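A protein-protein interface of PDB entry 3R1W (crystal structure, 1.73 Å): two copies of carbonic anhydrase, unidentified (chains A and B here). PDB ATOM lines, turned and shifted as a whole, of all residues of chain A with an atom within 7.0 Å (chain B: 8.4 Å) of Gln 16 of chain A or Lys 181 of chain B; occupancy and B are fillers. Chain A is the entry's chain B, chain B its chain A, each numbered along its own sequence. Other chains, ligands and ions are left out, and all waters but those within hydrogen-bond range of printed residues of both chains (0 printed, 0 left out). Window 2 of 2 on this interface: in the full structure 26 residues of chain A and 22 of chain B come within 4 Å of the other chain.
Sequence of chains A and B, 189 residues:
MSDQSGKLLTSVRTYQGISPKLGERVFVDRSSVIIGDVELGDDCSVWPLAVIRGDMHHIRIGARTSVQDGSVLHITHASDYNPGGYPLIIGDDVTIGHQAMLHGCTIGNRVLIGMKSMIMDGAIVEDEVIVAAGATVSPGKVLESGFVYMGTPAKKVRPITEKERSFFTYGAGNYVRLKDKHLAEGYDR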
ATOM      1  N   THR A  14     -16.172  11.106   7.870  1.00  0.00           N
ATOM      2  CA  THR A  14     -16.692  12.329   8.451  1.00  0.00           C
ATOM      3  C   THR A  14     -17.100  13.263   7.318  1.00  0.00           C
ATOM      4  O   THR A  14     -16.442  13.312   6.276  1.00  0.00           O
ATOM      5  CB  THR A  14     -15.610  12.992   9.307  1.00  0.00           C
ATOM      6  OG1 THR A  14     -15.303  12.129  10.409  1.00  0.00           O
ATOM      7  CG2 THR A  14     -16.074  14.342   9.829  1.00  0.00           C
ATOM      8  N   TYR A  15     -18.187  13.993   7.526  1.00  0.00           N
ATOM      9  CA  TYR A  15     -18.728  14.903   6.520  1.00  0.00           C
ATOM     10  C   TYR A  15     -19.269  16.145   7.219  1.00  0.00           C
ATOM     11  O   TYR A  15     -20.150  16.048   8.084  1.00  0.00           O
ATOM     12  CB  TYR A  15     -19.860  14.219   5.748  1.00  0.00           C
ATOM     13  CG  TYR A  15     -20.527  15.104   4.722  1.00  0.00           C
ATOM     14  CD1 TYR A  15     -19.919  15.351   3.497  1.00  0.00           C
ATOM     15  CD2 TYR A  15     -21.762  15.693   4.977  1.00  0.00           C
ATOM     16  CE1 TYR A  15     -20.523  16.165   2.546  1.00  0.00           C
ATOM     17  CE2 TYR A  15     -22.375  16.510   4.028  1.00  0.00           C
ATOM     18  CZ  TYR A  15     -21.749  16.739   2.819  1.00  0.00           C
ATOM     19  OH  TYR A  15     -22.352  17.540   1.878  1.00  0.00           O
ATOM     20  N   GLN A  16     -18.743  17.307   6.836  1.00  0.00           N
ATOM     21  CA  GLN A  16     -19.169  18.576   7.417  1.00  0.00           C
ATOM     22  C   GLN A  16     -19.213  18.512   8.933  1.00  0.00           C
ATOM     23  O   GLN A  16     -20.194  18.928   9.559  1.00  0.00           O
ATOM     24  CB  GLN A  16     -20.522  18.997   6.855  1.00  0.00           C
ATOM     25  CG  GLN A  16     -20.495  19.210   5.357  1.00  0.00           C
ATOM     26  CD  GLN A  16     -21.355  20.382   4.932  1.00  0.00           C
ATOM     27  OE1 GLN A  16     -22.584  20.327   5.006  1.00  0.00           O
ATOM     28  NE2 GLN A  16     -20.712  21.457   4.494  1.00  0.00           N
ATOM     29  N   GLY A  17     -18.149  17.972   9.512  1.00  0.00           N
ATOM     30  CA  GLY A  17     -18.006  17.912  10.960  1.00  0.00           C
ATOM     31  C   GLY A  17     -18.765  16.790  11.655  1.00  0.00           C
ATOM     32  O   GLY A  17     -18.676  16.645  12.872  1.00  0.00           O
ATOM     33  N   ILE A  18     -19.513  15.996  10.893  1.00  0.00           N
ATOM     34  CA  ILE A  18     -20.283  14.903  11.483  1.00  0.00           C
ATOM     35  C   ILE A  18     -19.687  13.552  11.124  1.00  0.00           C
ATOM     36  O   ILE A  18     -19.506  13.247   9.948  1.00  0.00           O
ATOM     37  CB  ILE A  18     -21.738  14.909  11.005  1.00  0.00           C
ATOM     38  CG1 ILE A  18     -22.349  16.302  11.161  1.00  0.00           C
ATOM     39  CG2 ILE A  18     -22.539  13.850  11.762  1.00  0.00           C
ATOM     40  CD1 ILE A  18     -23.587  16.511  10.327  1.00  0.00           C
ATOM     41  N   SER A  19     -19.397  12.742  12.142  1.00  0.00           N
ATOM     42  CA  SER A  19     -18.841  11.407  11.929  1.00  0.00           C
ATOM     43  C   SER A  19     -19.900  10.356  12.230  1.00  0.00           C
ATOM     44  O   SER A  19     -20.659  10.497  13.196  1.00  0.00           O
ATOM     45  CB  SER A  19     -17.630  11.177  12.832  1.00  0.00           C
ATOM     46  OG  SER A  19     -16.639  12.175  12.642  1.00  0.00           O
ATOM     47  N   GLY A  36     -21.078  10.605   6.865  1.00  0.00           N
ATOM     48  CA  GLY A  36     -21.776  11.661   7.582  1.00  0.00           C
ATOM     49  C   GLY A  36     -22.706  11.256   8.705  1.00  0.00           C
ATOM     50  O   GLY A  36     -22.302  10.560   9.640  1.00  0.00           O
ATOM     51  N   ASP A  55     -25.599  12.625   3.943  1.00  0.00           N
ATOM     52  CA  ASP A  55     -25.041  13.963   3.778  1.00  0.00           C
ATOM     53  C   ASP A  55     -26.088  15.062   3.971  1.00  0.00           C
ATOM     54  O   ASP A  55     -25.882  15.986   4.756  1.00  0.00           O
ATOM     55  CB  ASP A  55     -24.266  14.115   2.455  1.00  0.00           C
ATOM     56  CG  ASP A  55     -25.009  13.571   1.239  1.00  0.00           C
ATOM     57  OD1 ASP A  55     -26.214  13.221   1.329  1.00  0.00           O
ATOM     58  OD2 ASP A  55     -24.356  13.509   0.170  1.00  0.00           O
ATOM     59  N   MET A  56     -27.217  14.944   3.283  1.00  0.00           N
ATOM     60  CA  MET A  56     -28.238  15.991   3.322  1.00  0.00           C
ATOM     61  C   MET A  56     -29.348  15.762   4.348  1.00  0.00           C
ATOM     62  O   MET A  56     -30.240  16.586   4.489  1.00  0.00           O
ATOM     63  CB  MET A  56     -28.832  16.200   1.926  1.00  0.00           C
ATOM     64  CG  MET A  56     -27.792  16.637   0.905  1.00  0.00           C
ATOM     65  SD  MET A  56     -28.515  16.833  -0.731  1.00  0.00           S
ATOM     66  CE  MET A  56     -28.870  15.131  -1.168  1.00  0.00           C
ATOM     67  N   PHE B  27     -16.272  16.291  -9.679  1.00  0.00           N
ATOM     68  CA  PHE B  27     -16.095  15.434  -8.510  1.00  0.00           C
ATOM     69  C   PHE B  27     -16.209  13.979  -8.927  1.00  0.00           C
ATOM     70  O   PHE B  27     -17.222  13.568  -9.498  1.00  0.00           O
ATOM     71  CB  PHE B  27     -17.155  15.722  -7.435  1.00  0.00           C
ATOM     72  CG  PHE B  27     -17.156  14.718  -6.309  1.00  0.00           C
ATOM     73  CD1 PHE B  27     -16.019  14.546  -5.525  1.00  0.00           C
ATOM     74  CD2 PHE B  27     -18.279  13.941  -6.038  1.00  0.00           C
ATOM     75  CE1 PHE B  27     -15.997  13.618  -4.477  1.00  0.00           C
ATOM     76  CE2 PHE B  27     -18.267  13.013  -4.995  1.00  0.00           C
ATOM     77  CZ  PHE B  27     -17.122  12.855  -4.214  1.00  0.00           C
ATOM     78  N   TRP B  47     -20.579   9.574  -8.132  1.00  0.00           N
ATOM     79  CA  TRP B  47     -20.778   9.310  -6.707  1.00  0.00           C
ATOM     80  C   TRP B  47     -20.258   7.922  -6.302  1.00  0.00           C
ATOM     81  O   TRP B  47     -19.838   7.142  -7.163  1.00  0.00           O
ATOM     82  CB  TRP B  47     -22.254   9.563  -6.351  1.00  0.00           C
ATOM     83  CG  TRP B  47     -22.558  11.028  -6.573  1.00  0.00           C
ATOM     84  CD1 TRP B  47     -22.947  11.627  -7.746  1.00  0.00           C
ATOM     85  CD2 TRP B  47     -22.379  12.089  -5.622  1.00  0.00           C
ATOM     86  NE1 TRP B  47     -23.064  12.992  -7.565  1.00  0.00           N
ATOM     87  CE2 TRP B  47     -22.711  13.299  -6.277  1.00  0.00           C
ATOM     88  CE3 TRP B  47     -21.993  12.130  -4.278  1.00  0.00           C
ATOM     89  CZ2 TRP B  47     -22.678  14.530  -5.625  1.00  0.00           C
ATOM     90  CZ3 TRP B  47     -21.946  13.350  -3.641  1.00  0.00           C
ATOM     91  CH2 TRP B  47     -22.293  14.539  -4.311  1.00  0.00           C
ATOM     92  N   ASN B 174     -28.674  21.649  -7.120  1.00  0.00           N
ATOM     93  CA  ASN B 174     -28.447  21.131  -5.783  1.00  0.00           C
ATOM     94  C   ASN B 174     -27.283  20.134  -5.746  1.00  0.00           C
ATOM     95  O   ASN B 174     -26.465  20.156  -4.826  1.00  0.00           O
ATOM     96  CB  ASN B 174     -29.710  20.498  -5.214  1.00  0.00           C
ATOM     97  CG  ASN B 174     -29.499  19.994  -3.812  1.00  0.00           C
ATOM     98  OD1 ASN B 174     -29.172  20.766  -2.911  1.00  0.00           O
ATOM     99  ND2 ASN B 174     -29.650  18.694  -3.625  1.00  0.00           N
ATOM    100  N   TYR B 175     -27.204  19.267  -6.747  1.00  0.00           N
ATOM    101  CA  TYR B 175     -26.087  18.325  -6.810  1.00  0.00           C
ATOM    102  C   TYR B 175     -24.749  19.003  -7.111  1.00  0.00           C
ATOM    103  O   TYR B 175     -23.710  18.546  -6.642  1.00  0.00           O
ATOM    104  CB  TYR B 175     -26.373  17.143  -7.750  1.00  0.00           C
ATOM    105  CG  TYR B 175     -26.758  15.925  -6.948  1.00  0.00           C
ATOM    106  CD1 TYR B 175     -25.842  14.894  -6.726  1.00  0.00           C
ATOM    107  CD2 TYR B 175     -28.003  15.851  -6.335  1.00  0.00           C
ATOM    108  CE1 TYR B 175     -26.187  13.795  -5.942  1.00  0.00           C
ATOM    109  CE2 TYR B 175     -28.352  14.761  -5.552  1.00  0.00           C
ATOM    110  CZ  TYR B 175     -27.443  13.744  -5.363  1.00  0.00           C
ATOM    111  OH  TYR B 175     -27.794  12.665  -4.588  1.00  0.00           O
ATOM    112  N   VAL B 176     -24.775  20.103  -7.862  1.00  0.00           N
ATOM    113  CA  VAL B 176     -23.561  20.879  -8.073  1.00  0.00           C
ATOM    114  C   VAL B 176     -23.032  21.414  -6.729  1.00  0.00           C
ATOM    115  O   VAL B 176     -21.855  21.259  -6.402  1.00  0.00           O
ATOM    116  CB  VAL B 176     -23.794  22.032  -9.066  1.00  0.00           C
ATOM    117  CG1 VAL B 176     -22.618  23.027  -9.039  1.00  0.00           C
ATOM    118  CG2 VAL B 176     -24.000  21.471 -10.475  1.00  0.00           C
ATOM    119  N   ARG B 177     -23.916  22.019  -5.942  1.00  0.00           N
ATOM    120  CA  ARG B 177     -23.521  22.500  -4.623  1.00  0.00           C
ATOM    121  C   ARG B 177     -23.097  21.348  -3.707  1.00  0.00           C
ATOM    122  O   ARG B 177     -22.151  21.481  -2.933  1.00  0.00           O
ATOM    123  CB  ARG B 177     -24.650  23.325  -3.991  1.00  0.00           C
ATOM    124  CG  ARG B 177     -24.895  24.644  -4.745  1.00  0.00           C
ATOM    125  CD  ARG B 177     -26.007  25.490  -4.115  1.00  0.00           C
ATOM    126  NE  ARG B 177     -27.344  25.078  -4.549  1.00  0.00           N
ATOM    127  CZ  ARG B 177     -28.260  24.531  -3.754  1.00  0.00           C
ATOM    128  NH1 ARG B 177     -27.998  24.328  -2.468  1.00  0.00           N
ATOM    129  NH2 ARG B 177     -29.450  24.196  -4.238  1.00  0.00           N
ATOM    130  N   LEU B 178     -23.779  20.214  -3.816  1.00  0.00           N
ATOM    131  CA  LEU B 178     -23.449  19.062  -2.988  1.00  0.00           C
ATOM    132  C   LEU B 178     -22.077  18.487  -3.346  1.00  0.00           C
ATOM    133  O   LEU B 178     -21.292  18.167  -2.451  1.00  0.00           O
ATOM    134  CB  LEU B 178     -24.510  17.975  -3.116  1.00  0.00           C
ATOM    135  CG  LEU B 178     -24.320  16.778  -2.185  1.00  0.00           C
ATOM    136  CD1 LEU B 178     -24.507  17.184  -0.716  1.00  0.00           C
ATOM    137  CD2 LEU B 178     -25.283  15.689  -2.583  1.00  0.00           C
ATOM    138  N   LYS B 179     -21.770  18.369  -4.639  1.00  0.00           N
ATOM    139  CA  LYS B 179     -20.462  17.804  -4.999  1.00  0.00           C
ATOM    140  C   LYS B 179     -19.330  18.746  -4.584  1.00  0.00           C
ATOM    141  O   LYS B 179     -18.217  18.311  -4.339  1.00  0.00           O
ATOM    142  CB  LYS B 179     -20.363  17.347  -6.478  1.00  0.00           C
ATOM    143  CG  LYS B 179     -20.572  18.419  -7.558  1.00  0.00           C
ATOM    144  CD  LYS B 179     -19.318  19.233  -7.844  1.00  0.00           C
ATOM    145  CE  LYS B 179     -19.644  20.406  -8.778  1.00  0.00           C
ATOM    146  NZ  LYS B 179     -18.483  21.309  -9.004  1.00  0.00           N
ATOM    147  N   ASP B 180     -19.625  20.037  -4.472  1.00  0.00           N
ATOM    148  CA  ASP B 180     -18.601  20.973  -4.028  1.00  0.00           C
ATOM    149  C   ASP B 180     -18.271  20.731  -2.554  1.00  0.00           C
ATOM    150  O   ASP B 180     -17.123  20.884  -2.140  1.00  0.00           O
ATOM    151  CB  ASP B 180     -19.009  22.422  -4.293  1.00  0.00           C
ATOM    152  CG  ASP B 180     -18.863  22.808  -5.769  1.00  0.00           C
ATOM    153  OD1 ASP B 180     -17.986  22.241  -6.453  1.00  0.00           O
ATOM    154  OD2 ASP B 180     -19.617  23.688  -6.234  1.00  0.00           O
ATOM    155  N   LYS B 181     -19.277  20.322  -1.781  1.00  0.00           N
ATOM    156  CA  LYS B 181     -19.068  19.960  -0.378  1.00  0.00           C
ATOM    157  C   LYS B 181     -18.254  18.676  -0.244  1.00  0.00           C
ATOM    158  O   LYS B 181     -17.381  18.566   0.618  1.00  0.00           O
ATOM    159  CB  LYS B 181     -20.398  19.818   0.361  1.00  0.00           C
ATOM    160  CG  LYS B 181     -21.126  21.137   0.552  1.00  0.00           C
ATOM    161  CD  LYS B 181     -22.442  20.943   1.282  1.00  0.00           C
ATOM    162  CE  LYS B 181     -23.237  22.240   1.339  1.00  0.00           C
ATOM    163  NZ  LYS B 181     -24.489  22.066   2.132  1.00  0.00           N
ATOM    164  N   HIS B 182     -18.553  17.699  -1.094  1.00  0.00           N
ATOM    165  CA  HIS B 182     -17.812  16.445  -1.096  1.00  0.00           C
ATOM    166  C   HIS B 182     -16.374  16.648  -1.551  1.00  0.00           C
ATOM    167  O   HIS B 182     -15.457  16.005  -1.018  1.00  0.00           O
ATOM    168  CB  HIS B 182     -18.513  15.395  -1.959  1.00  0.00           C
ATOM    169  CG  HIS B 182     -19.643  14.700  -1.262  1.00  0.00           C
ATOM    170  ND1 HIS B 182     -20.806  15.345  -0.889  1.00  0.00           N
ATOM    171  CD2 HIS B 182     -19.778  13.418  -0.865  1.00  0.00           C
ATOM    172  CE1 HIS B 182     -21.614  14.481  -0.298  1.00  0.00           C
ATOM    173  NE2 HIS B 182     -21.013  13.303  -0.275  1.00  0.00           N
ATOM    174  N   LEU B 183     -16.171  17.561  -2.504  1.00  0.00           N
ATOM    175  CA  LEU B 183     -14.826  17.920  -2.939  1.00  0.00           C
ATOM    176  C   LEU B 183     -14.080  18.561  -1.785  1.00  0.00           C
ATOM    177  O   LEU B 183     -12.889  18.308  -1.597  1.00  0.00           O
ATOM    178  CB  LEU B 183     -14.857  18.894  -4.117  1.00  0.00           C
ATOM    179  CG  LEU B 183     -15.120  18.271  -5.487  1.00  0.00           C
ATOM    180  CD1 LEU B 183     -15.518  19.333  -6.495  1.00  0.00           C
ATOM    181  CD2 LEU B 183     -13.881  17.506  -5.967  1.00  0.00           C
ATOM    182  N   ALA B 184     -14.782  19.402  -1.027  1.00  0.00           N
ATOM    183  CA  ALA B 184     -14.170  20.089   0.108  1.00  0.00           C
ATOM    184  C   ALA B 184     -13.783  19.124   1.224  1.00  0.00           C
ATOM    185  O   ALA B 184     -12.884  19.416   2.018  1.00  0.00           O
ATOM    186  CB  ALA B 184     -15.087  21.194   0.636  1.00  0.00           C
ATOM    187  N   GLU B 185     -14.452  17.973   1.295  1.00  0.00           N
ATOM    188  CA  GLU B 185     -14.072  16.956   2.276  1.00  0.00           C
ATOM    189  C   GLU B 185     -12.897  16.120   1.788  1.00  0.00           C
ATOM    190  O   GLU B 185     -12.377  15.295   2.541  1.00  0.00           O
ATOM    191  CB  GLU B 185     -15.232  16.013   2.614  1.00  0.00           C
ATOM    192  CG  GLU B 185     -16.391  16.639   3.336  1.00  0.00           C
ATOM    193  CD  GLU B 185     -16.095  17.037   4.780  1.00  0.00           C
ATOM    194  OE1 GLU B 185     -15.194  16.470   5.454  1.00  0.00           O
ATOM    195  OE2 GLU B 185     -16.807  17.925   5.254  1.00  0.00           O
ATOM    196  N   GLY B 186     -12.503  16.327   0.530  1.00  0.00           N
ATOM    197  CA  GLY B 186     -11.401  15.601  -0.090  1.00  0.00           C
ATOM    198  C   GLY B 186     -11.713  14.172  -0.514  1.00  0.00           C
ATOM    199  O   GLY B 186     -10.806  13.346  -0.592  1.00  0.00           O
ATOM    200  N   TYR B 187     -12.988  13.878  -0.786  1.00  0.00           N
ATOM    201  CA  TYR B 187     -13.412  12.503  -1.076  1.00  0.00           C
ATOM    202  C   TYR B 187     -12.911  11.964  -2.415  1.00  0.00           C
ATOM    203  O   TYR B 187     -13.032  10.762  -2.678  1.00  0.00           O
ATOM    204  CB  TYR B 187     -14.938  12.362  -1.051  1.00  0.00           C
ATOM    205  CG  TYR B 187     -15.597  12.421   0.309  1.00  0.00           C
ATOM    206  CD1 TYR B 187     -14.856  12.372   1.494  1.00  0.00           C
ATOM    207  CD2 TYR B 187     -16.977  12.501   0.406  1.00  0.00           C
ATOM    208  CE1 TYR B 187     -15.501  12.410   2.747  1.00  0.00           C
ATOM    209  CE2 TYR B 187     -17.621  12.546   1.624  1.00  0.00           C
ATOM    210  CZ  TYR B 187     -16.882  12.506   2.794  1.00  0.00           C
ATOM    211  OH  TYR B 187     -17.556  12.556   3.995  1.00  0.00           O
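Of chain B, only Lys 181 (3.7 Å) and Glu 185 (2.6 Å) come within 4 Å of Gln 16 of chain A. Of the printed residues of chain A, Lys 181 of chain B touches Tyr 15 (3.4 Å) and Gln 16 (3.7 Å). No residue of chain B comes within 4 Å of Gly 17 of chain A. Printed residues of chain B within 4 Å of Met 56 of chain A: Asn 174 (3.6 Å) and Leu 178 (3.7 Å). Of the printed residues of chain A, Leu 178 of chain B touches Tyr 15, Asp 55 and Met 56. The nearest residue of chain B that does not touch Gln 16 of chain A is Tyr 187 of chain B (5.7 Å). The nearest printed residue of chain A that does not touch Asn 174 of chain B is Asp 55 of chain A (8.1 Å).
Among the printed residues, merely in contact across the chains: Tyr 15 of chain A with Leu 178 of chain B (3.4 Å), Tyr 15 of chain A with Lys 181 of chain B (3.4 Å), Tyr 15 of chain A with His 182 of chain B (3.5 Å), Tyr 15 of chain A with Glu 185 of chain B (3.6 Å), Tyr 15 of chain A with Tyr 187 of chain B (3.3 Å), Gln 16 of chain A with Lys 181 of chain B (3.7 Å), Asp 55 of chain A with Leu 178 of chain B (3.6 Å) and Met 56 of chain A with Leu 178 of chain B (3.7 Å).
O of Leu 178 of chain B is in hydrogen-bond range of ND1 of His 182 of chain B, 3.3 Å away. The backbone carbonyl oxygen of His 182 of chain B is in hydrogen-bond range of the backbone NH of Tyr 187 of chain B, at 3.3 Å. The side-chain hydroxyl (OG1) of Thr 14 of chain A lies within hydrogen-bond range of the side-chain hydroxyl (OG) of Ser 19 of chain A (2.6 Å).
Hydrophobic or aromatic side chains of chain B within 4 Å of the printed part of chain A: Leu 178, His 182 and Tyr 187. Of the 9 printed residues of chain A, 5 touch a printed residue of chain B. Hydrophobic or aromatic side chains of chain A within 4 Å of the printed part of chain B: Tyr 15 and Met 56. Among the printed residues, 13 pairs touch across the chains.
No position is printed for both chains. Of the 13 pairs that touch across the chains among the printed residues, none has its exchanged pair printed and touching as well.
The side-chain amide nitrogen (ND2) of Asn 174 of chain B sits at hydrogen-bond distance from the side-chain sulfur (SD) of Met 56 of chain A. A ring nitrogen (NE2) of His 182 of chain B lies close to the side-chain carboxylate of Asp 55 of chain A. OE2 of Glu 185 of chain B sits at hydrogen-bond distance from N of Gln 16 of chain A, 2.6 Å away. O of Thr 14 of chain A is in hydrogen-bond range of OH of Tyr 187 of chain B (2.6 Å). The backbone carbonyl oxygen (O) of Thr 14 of chain A lies close to the side-chain carboxylate (OE1) of Glu 185 of chain B (3.5 Å).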
